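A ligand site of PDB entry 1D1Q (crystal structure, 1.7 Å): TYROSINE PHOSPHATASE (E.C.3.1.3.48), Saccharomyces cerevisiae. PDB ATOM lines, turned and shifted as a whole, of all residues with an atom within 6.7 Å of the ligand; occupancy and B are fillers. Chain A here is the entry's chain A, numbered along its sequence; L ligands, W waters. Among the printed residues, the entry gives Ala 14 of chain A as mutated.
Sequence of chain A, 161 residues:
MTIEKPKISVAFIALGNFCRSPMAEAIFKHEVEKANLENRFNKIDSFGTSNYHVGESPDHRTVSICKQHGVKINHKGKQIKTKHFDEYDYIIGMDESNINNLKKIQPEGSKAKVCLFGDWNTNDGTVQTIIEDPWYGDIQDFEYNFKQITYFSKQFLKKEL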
ATOM      1  N   ILE A  13      32.445 -23.964  19.315  1.00  0.00           N
ATOM      2  CA  ILE A  13      31.888 -25.293  19.522  1.00  0.00           C
ATOM      3  C   ILE A  13      30.383 -25.405  19.315  1.00  0.00           C
ATOM      4  O   ILE A  13      29.615 -24.554  19.767  1.00  0.00           O
ATOM      5  CB  ILE A  13      32.141 -25.787  21.008  1.00  0.00           C
ATOM      6  CG1 ILE A  13      33.561 -25.414  21.463  1.00  0.00           C
ATOM      7  CG2 ILE A  13      31.823 -27.287  21.155  1.00  0.00           C
ATOM      8  CD1 ILE A  13      34.681 -26.166  20.726  1.00  0.00           C
ATOM      9  N   ALA A  14      29.965 -26.459  18.640  1.00  0.00           N
ATOM     10  CA  ALA A  14      28.531 -26.708  18.556  1.00  0.00           C
ATOM     11  C   ALA A  14      28.387 -28.230  18.765  1.00  0.00           C
ATOM     12  O   ALA A  14      29.275 -28.870  19.357  1.00  0.00           O
ATOM     13  CB  ALA A  14      27.955 -26.258  17.209  1.00  0.00           C
ATOM     14  N   LEU A  15      27.293 -28.841  18.323  1.00  0.00           N
ATOM     15  CA  LEU A  15      27.155 -30.287  18.544  1.00  0.00           C
ATOM     16  C   LEU A  15      27.868 -31.083  17.437  1.00  0.00           C
ATOM     17  O   LEU A  15      28.744 -31.906  17.727  1.00  0.00           O
ATOM     18  CB  LEU A  15      25.666 -30.682  18.605  1.00  0.00           C
ATOM     19  CG  LEU A  15      25.385 -32.186  18.504  1.00  0.00           C
ATOM     20  CD1 LEU A  15      25.913 -32.898  19.731  1.00  0.00           C
ATOM     21  CD2 LEU A  15      23.872 -32.412  18.356  1.00  0.00           C
ATOM     22  N   GLY A  16      27.497 -30.838  16.176  1.00  0.00           N
ATOM     23  CA  GLY A  16      28.114 -31.588  15.100  1.00  0.00           C
ATOM     24  C   GLY A  16      29.321 -30.982  14.394  1.00  0.00           C
ATOM     25  O   GLY A  16      29.998 -31.736  13.684  1.00  0.00           O
ATOM     26  N   ASN A  17      29.629 -29.684  14.602  1.00  0.00           N
ATOM     27  CA  ASN A  17      30.726 -29.023  13.855  1.00  0.00           C
ATOM     28  C   ASN A  17      30.367 -29.228  12.379  1.00  0.00           C
ATOM     29  O   ASN A  17      31.194 -29.685  11.573  1.00  0.00           O
ATOM     30  CB  ASN A  17      32.082 -29.669  14.145  1.00  0.00           C
ATOM     31  CG  ASN A  17      33.251 -28.855  13.591  1.00  0.00           C
ATOM     32  OD1 ASN A  17      34.290 -29.400  13.250  1.00  0.00           O
ATOM     33  ND2 ASN A  17      33.077 -27.521  13.528  1.00  0.00           N
ATOM     34  N   PHE A  18      29.121 -28.890  12.044  1.00  0.00           N
ATOM     35  CA  PHE A  18      28.558 -29.127  10.716  1.00  0.00           C
ATOM     36  C   PHE A  18      27.737 -27.934  10.255  1.00  0.00           C
ATOM     37  O   PHE A  18      27.858 -27.512   9.109  1.00  0.00           O
ATOM     38  CB  PHE A  18      27.683 -30.403  10.791  1.00  0.00           C
ATOM     39  CG  PHE A  18      27.274 -30.982   9.455  1.00  0.00           C
ATOM     40  CD1 PHE A  18      28.222 -31.328   8.507  1.00  0.00           C
ATOM     41  CD2 PHE A  18      25.915 -31.205   9.165  1.00  0.00           C
ATOM     42  CE1 PHE A  18      27.843 -31.907   7.282  1.00  0.00           C
ATOM     43  CE2 PHE A  18      25.518 -31.784   7.944  1.00  0.00           C
ATOM     44  CZ  PHE A  18      26.486 -32.139   7.004  1.00  0.00           C
ATOM     45  N   CYS A  19      26.906 -27.379  11.137  1.00  0.00           N
ATOM     46  CA  CYS A  19      26.093 -26.211  10.765  1.00  0.00           C
ATOM     47  C   CYS A  19      26.658 -24.936  11.378  1.00  0.00           C
ATOM     48  O   CYS A  19      27.289 -24.134  10.710  1.00  0.00           O
ATOM     49  CB  CYS A  19      24.629 -26.382  11.194  1.00  0.00           C
ATOM     50  SG  CYS A  19      23.748 -27.725  10.336  1.00  0.00           S
ATOM     51  N   ARG A  20      26.453 -24.756  12.672  1.00  0.00           N
ATOM     52  CA  ARG A  20      26.858 -23.501  13.279  1.00  0.00           C
ATOM     53  C   ARG A  20      28.341 -23.232  13.540  1.00  0.00           C
ATOM     54  O   ARG A  20      28.834 -22.129  13.200  1.00  0.00           O
ATOM     55  CB  ARG A  20      26.104 -23.294  14.601  1.00  0.00           C
ATOM     56  CG  ARG A  20      24.576 -23.170  14.446  1.00  0.00           C
ATOM     57  CD  ARG A  20      23.899 -23.534  15.764  1.00  0.00           C
ATOM     58  NE  ARG A  20      24.137 -24.941  16.120  1.00  0.00           N
ATOM     59  CZ  ARG A  20      23.821 -25.467  17.311  1.00  0.00           C
ATOM     60  NH1 ARG A  20      23.259 -24.715  18.258  1.00  0.00           N
ATOM     61  NH2 ARG A  20      24.054 -26.759  17.548  1.00  0.00           N
ATOM     62  N   SER A  21      29.065 -24.178  14.132  1.00  0.00           N
ATOM     63  CA  SER A  21      30.433 -23.840  14.472  1.00  0.00           C
ATOM     64  C   SER A  21      31.355 -23.585  13.269  1.00  0.00           C
ATOM     65  O   SER A  21      32.218 -22.685  13.351  1.00  0.00           O
ATOM     66  CB  SER A  21      31.037 -24.801  15.526  1.00  0.00           C
ATOM     67  OG  SER A  21      31.078 -26.155  15.123  1.00  0.00           O
ATOM     68  N   PRO A  22      31.223 -24.350  12.162  1.00  0.00           N
ATOM     69  CA  PRO A  22      32.088 -24.050  11.006  1.00  0.00           C
ATOM     70  C   PRO A  22      31.743 -22.625  10.507  1.00  0.00           C
ATOM     71  O   PRO A  22      32.621 -21.865  10.050  1.00  0.00           O
ATOM     72  CB  PRO A  22      31.714 -25.131   9.973  1.00  0.00           C
ATOM     73  CG  PRO A  22      31.174 -26.287  10.846  1.00  0.00           C
ATOM     74  CD  PRO A  22      30.386 -25.550  11.923  1.00  0.00           C
ATOM     75  N   PHE A  47      34.959 -26.888  16.269  1.00  0.00           N
ATOM     76  CA  PHE A  47      34.844 -28.284  16.659  1.00  0.00           C
ATOM     77  C   PHE A  47      33.408 -28.591  17.039  1.00  0.00           C
ATOM     78  O   PHE A  47      32.530 -27.696  17.087  1.00  0.00           O
ATOM     79  CB  PHE A  47      35.668 -28.575  17.936  1.00  0.00           C
ATOM     80  CG  PHE A  47      37.131 -28.309  17.826  1.00  0.00           C
ATOM     81  CD1 PHE A  47      37.648 -27.037  18.066  1.00  0.00           C
ATOM     82  CD2 PHE A  47      38.026 -29.355  17.558  1.00  0.00           C
ATOM     83  CE1 PHE A  47      39.048 -26.790  18.047  1.00  0.00           C
ATOM     84  CE2 PHE A  47      39.426 -29.121  17.537  1.00  0.00           C
ATOM     85  CZ  PHE A  47      39.926 -27.835  17.783  1.00  0.00           C
ATOM     86  N   GLY A  48      33.167 -29.866  17.380  1.00  0.00           N
ATOM     87  CA  GLY A  48      31.850 -30.254  17.834  1.00  0.00           C
ATOM     88  C   GLY A  48      32.051 -31.083  19.091  1.00  0.00           C
ATOM     89  O   GLY A  48      33.151 -31.629  19.326  1.00  0.00           O
ATOM     90  N   TYR A  52      29.926 -37.057  15.251  1.00  0.00           N
ATOM     91  CA  TYR A  52      28.986 -37.402  14.162  1.00  0.00           C
ATOM     92  C   TYR A  52      29.303 -36.918  12.747  1.00  0.00           C
ATOM     93  O   TYR A  52      28.846 -37.528  11.770  1.00  0.00           O
ATOM     94  CB  TYR A  52      27.568 -36.929  14.516  1.00  0.00           C
ATOM     95  CG  TYR A  52      27.043 -37.457  15.835  1.00  0.00           C
ATOM     96  CD1 TYR A  52      26.372 -36.612  16.724  1.00  0.00           C
ATOM     97  CD2 TYR A  52      27.249 -38.789  16.220  1.00  0.00           C
ATOM     98  CE1 TYR A  52      25.930 -37.073  17.967  1.00  0.00           C
ATOM     99  CE2 TYR A  52      26.803 -39.266  17.470  1.00  0.00           C
ATOM    100  CZ  TYR A  52      26.151 -38.396  18.337  1.00  0.00           C
ATOM    101  OH  TYR A  52      25.715 -38.837  19.586  1.00  0.00           O
ATOM    102  N   HIS A  53      30.089 -35.857  12.617  1.00  0.00           N
ATOM    103  CA  HIS A  53      30.430 -35.328  11.295  1.00  0.00           C
ATOM    104  C   HIS A  53      31.930 -35.168  11.122  1.00  0.00           C
ATOM    105  O   HIS A  53      32.397 -34.356  10.318  1.00  0.00           O
ATOM    106  CB  HIS A  53      29.698 -34.008  11.075  1.00  0.00           C
ATOM    107  CG  HIS A  53      28.202 -34.163  11.042  1.00  0.00           C
ATOM    108  ND1 HIS A  53      27.532 -34.530   9.893  1.00  0.00           N
ATOM    109  CD2 HIS A  53      27.281 -34.121  12.030  1.00  0.00           C
ATOM    110  CE1 HIS A  53      26.251 -34.712  10.181  1.00  0.00           C
ATOM    111  NE2 HIS A  53      26.079 -34.466  11.464  1.00  0.00           N
ATOM    112  N   ASP A  59      27.627 -28.391   6.419  1.00  0.00           N
ATOM    113  CA  ASP A  59      26.293 -28.543   5.842  1.00  0.00           C
ATOM    114  C   ASP A  59      26.192 -27.618   4.618  1.00  0.00           C
ATOM    115  O   ASP A  59      26.623 -26.443   4.667  1.00  0.00           O
ATOM    116  CB  ASP A  59      25.246 -28.164   6.883  1.00  0.00           C
ATOM    117  CG  ASP A  59      23.831 -28.354   6.387  1.00  0.00           C
ATOM    118  OD1 ASP A  59      23.226 -29.397   6.707  1.00  0.00           O
ATOM    119  OD2 ASP A  59      23.303 -27.466   5.686  1.00  0.00           O
ATOM    120  N   MET A  94      27.612 -22.462  21.144  1.00  0.00           N
ATOM    121  CA  MET A  94      26.504 -21.786  20.439  1.00  0.00           C
ATOM    122  C   MET A  94      25.254 -21.665  21.327  1.00  0.00           C
ATOM    123  O   MET A  94      24.591 -20.622  21.322  1.00  0.00           O
ATOM    124  CB  MET A  94      26.128 -22.574  19.179  1.00  0.00           C
ATOM    125  CG  MET A  94      27.275 -22.786  18.180  1.00  0.00           C
ATOM    126  SD  MET A  94      27.914 -21.212  17.436  1.00  0.00           S
ATOM    127  CE  MET A  94      29.327 -20.880  18.498  1.00  0.00           C
ATOM    128  N   ASN A  98      25.471 -26.993  24.577  1.00  0.00           N
ATOM    129  CA  ASN A  98      26.898 -27.085  24.253  1.00  0.00           C
ATOM    130  C   ASN A  98      27.698 -26.772  25.539  1.00  0.00           C
ATOM    131  O   ASN A  98      28.660 -27.480  25.880  1.00  0.00           O
ATOM    132  CB  ASN A  98      27.297 -26.056  23.204  1.00  0.00           C
ATOM    133  CG  ASN A  98      26.562 -26.228  21.875  1.00  0.00           C
ATOM    134  OD1 ASN A  98      26.284 -25.251  21.196  1.00  0.00           O
ATOM    135  ND2 ASN A  98      26.248 -27.492  21.505  1.00  0.00           N
ATOM    136  N   GLU A 132      20.595 -20.651  17.913  1.00  0.00           N
ATOM    137  CA  GLU A 132      19.827 -21.882  17.854  1.00  0.00           C
ATOM    138  C   GLU A 132      20.176 -22.787  16.719  1.00  0.00           C
ATOM    139  O   GLU A 132      20.423 -22.318  15.590  1.00  0.00           O
ATOM    140  CB  GLU A 132      18.319 -21.587  17.817  1.00  0.00           C
ATOM    141  CG  GLU A 132      17.768 -21.021  19.163  1.00  0.00           C
ATOM    142  CD  GLU A 132      16.314 -20.650  19.082  1.00  0.00           C
ATOM    143  OE1 GLU A 132      15.584 -20.887  20.074  1.00  0.00           O
ATOM    144  OE2 GLU A 132      15.893 -20.124  18.031  1.00  0.00           O
ATOM    145  N   ASP A 133      20.168 -24.086  17.014  1.00  0.00           N
ATOM    146  CA  ASP A 133      20.444 -25.148  16.047  1.00  0.00           C
ATOM    147  C   ASP A 133      19.441 -24.985  14.885  1.00  0.00           C
ATOM    148  O   ASP A 133      18.217 -25.071  15.089  1.00  0.00           O
ATOM    149  CB  ASP A 133      20.263 -26.515  16.720  1.00  0.00           C
ATOM    150  CG  ASP A 133      20.612 -27.691  15.803  1.00  0.00           C
ATOM    151  OD1 ASP A 133      20.838 -27.476  14.601  1.00  0.00           O
ATOM    152  OD2 ASP A 133      20.661 -28.827  16.276  1.00  0.00           O
ATOM    153  N   PRO A 134      19.940 -24.698  13.667  1.00  0.00           N
ATOM    154  CA  PRO A 134      19.050 -24.528  12.511  1.00  0.00           C
ATOM    155  C   PRO A 134      18.701 -25.841  11.801  1.00  0.00           C
ATOM    156  O   PRO A 134      17.945 -25.822  10.816  1.00  0.00           O
ATOM    157  CB  PRO A 134      19.860 -23.622  11.583  1.00  0.00           C
ATOM    158  CG  PRO A 134      21.293 -24.153  11.799  1.00  0.00           C
ATOM    159  CD  PRO A 134      21.352 -24.458  13.313  1.00  0.00           C
ATOM    160  N   TRP A 135      19.232 -26.963  12.265  1.00  0.00           N
ATOM    161  CA  TRP A 135      19.024 -28.248  11.609  1.00  0.00           C
ATOM    162  C   TRP A 135      17.634 -28.566  11.053  1.00  0.00           C
ATOM    163  O   TRP A 135      17.480 -28.960   9.883  1.00  0.00           O
ATOM    164  CB  TRP A 135      19.438 -29.398  12.523  1.00  0.00           C
ATOM    165  CG  TRP A 135      19.399 -30.694  11.775  1.00  0.00           C
ATOM    166  CD1 TRP A 135      18.488 -31.723  11.931  1.00  0.00           C
ATOM    167  CD2 TRP A 135      20.282 -31.107  10.735  1.00  0.00           C
ATOM    168  NE1 TRP A 135      18.772 -32.740  11.060  1.00  0.00           N
ATOM    169  CE2 TRP A 135      19.871 -32.400  10.318  1.00  0.00           C
ATOM    170  CE3 TRP A 135      21.402 -30.513  10.122  1.00  0.00           C
ATOM    171  CZ2 TRP A 135      20.535 -33.094   9.303  1.00  0.00           C
ATOM    172  CZ3 TRP A 135      22.063 -31.222   9.113  1.00  0.00           C
ATOM    173  CH2 TRP A 135      21.630 -32.489   8.713  1.00  0.00           C
ATOM    174  N   TYR A 136      16.643 -28.415  11.914  1.00  0.00           N
ATOM    175  CA  TYR A 136      15.260 -28.702  11.562  1.00  0.00           C
ATOM    176  C   TYR A 136      14.533 -27.508  10.989  1.00  0.00           C
ATOM    177  O   TYR A 136      13.319 -27.552  10.796  1.00  0.00           O
ATOM    178  CB  TYR A 136      14.513 -29.184  12.813  1.00  0.00           C
ATOM    179  CG  TYR A 136      14.847 -30.614  13.120  1.00  0.00           C
ATOM    180  CD1 TYR A 136      15.587 -30.950  14.245  1.00  0.00           C
ATOM    181  CD2 TYR A 136      14.442 -31.623  12.259  1.00  0.00           C
ATOM    182  CE1 TYR A 136      15.921 -32.296  14.508  1.00  0.00           C
ATOM    183  CE2 TYR A 136      14.761 -32.959  12.505  1.00  0.00           C
ATOM    184  CZ  TYR A 136      15.505 -33.281  13.623  1.00  0.00           C
ATOM    185  OH  TYR A 136      15.823 -34.599  13.838  1.00  0.00           O
ATOM    186  N   ASN A 145      21.598 -17.202  11.832  1.00  0.00           N
ATOM    187  CA  ASN A 145      22.803 -17.578  12.583  1.00  0.00           C
ATOM    188  C   ASN A 145      23.988 -16.693  12.089  1.00  0.00           C
ATOM    189  O   ASN A 145      24.827 -16.231  12.873  1.00  0.00           O
ATOM    190  CB  ASN A 145      23.171 -19.043  12.319  1.00  0.00           C
ATOM    191  CG  ASN A 145      22.315 -20.051  13.106  1.00  0.00           C
ATOM    192  OD1 ASN A 145      21.625 -19.725  14.097  1.00  0.00           O
ATOM    193  ND2 ASN A 145      22.355 -21.284  12.651  1.00  0.00           N
HETATM  194  P1  LIG L   1      26.197 -27.861  14.588  1.00  0.00           P
HETATM  195  O1  LIG L   1      25.683 -28.961  13.427  1.00  0.00           O
HETATM  196  O2  LIG L   1      27.652 -27.679  14.234  1.00  0.00           O
HETATM  197  O3  LIG L   1      25.905 -28.501  15.940  1.00  0.00           O
HETATM  198  O4  LIG L   1      25.341 -26.654  14.356  1.00  0.00           O
HETATM  199  C1  LIG L   1      24.632 -29.818  13.522  1.00  0.00           C
HETATM  200  C2  LIG L   1      23.438 -29.402  14.152  1.00  0.00           C
HETATM  201  C3  LIG L   1      22.349 -30.289  14.259  1.00  0.00           C
HETATM  202  C4  LIG L   1      22.459 -31.585  13.740  1.00  0.00           C
HETATM  203  C5  LIG L   1      23.615 -32.021  13.102  1.00  0.00           C
HETATM  204  C6  LIG L   1      24.716 -31.140  12.987  1.00  0.00           C
HETATM  205  N1  LIG L   1      21.300 -32.511  13.878  1.00  0.00           N
HETATM  206  O5  LIG L   1      21.277 -33.489  13.153  1.00  0.00           O
HETATM  207  O6  LIG L   1      20.448 -32.257  14.714  1.00  0.00           O
HETATM  208  O   HOH W   1      18.611 -30.668  15.891  1.00  0.00           O
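Ala 14 touches the ligand (CB to O3, 3.3 Å).
Ser 21 touches the ligand (N to O2, 3.8 Å).
NE2 of His 53 touches C5 of the ligand, 3.8 Å away.
OD2 of Asp 133 touches C3 of the ligand, at 3.0 Å.
Hydrophobic or aromatic side chains within 4 Å of the ligand: Ala 14, Leu 15, Phe 18 and Trp 135.
The nearest printed residue that does not touch the ligand is Pro 22 (4.2 Å).
Water W1 lies within hydrogen-bond range of O6 of the ligand (2.7 Å) and OD2 of Asp 133 (2.8 Å).
The backbone carbonyl oxygen of Phe 47 sits at hydrogen-bond distance from the side-chain hydroxyl of Ser 21, 2.9 Å away.
The backbone NH of Ala 14 sits at hydrogen-bond distance from the backbone carbonyl oxygen of Phe 47, at 3.2 Å.
The side-chain hydroxyl (OG) of Ser 21 lies within hydrogen-bond range of the side-chain amide nitrogen (ND2) of Asn 17, at 2.9 Å.
ND2 of Asn 17 sits close to N of Phe 47, at 3.4 Å.
N of Asp 59 lies within hydrogen-bond range of O of Phe 18, 2.8 Å away.
OD1 of Asp 133 lies within hydrogen-bond range of N of Trp 135, 2.9 Å away.
An oxygen (O4) of the ligand lies within salt-bridge range of the guanidinium group (NE) of Arg 20.
The backbone NH (N) of Asn 17 sits at hydrogen-bond distance from an oxygen (O2) of the ligand (2.8 Å).
An oxygen (O3) of the ligand is in hydrogen-bond range of the backbone NH (N) of Leu 15 (2.8 Å).
The indole nitrogen (NE1) of Trp 135 lies close to an oxygen (O5) of the ligand, at 3.3 Å.
The backbone NH of Cys 19 is in hydrogen-bond range of an oxygen (O1) of the ligand (3.0 Å).
N of Arg 20 lies within hydrogen-bond range of O4 of the ligand (2.8 Å).
The backbone NH (N) of Phe 18 lies within hydrogen-bond range of an oxygen (O2) of the ligand.
The backbone NH of Gly 16 is in hydrogen-bond range of an oxygen (O3) of the ligand, at 2.8 Å.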
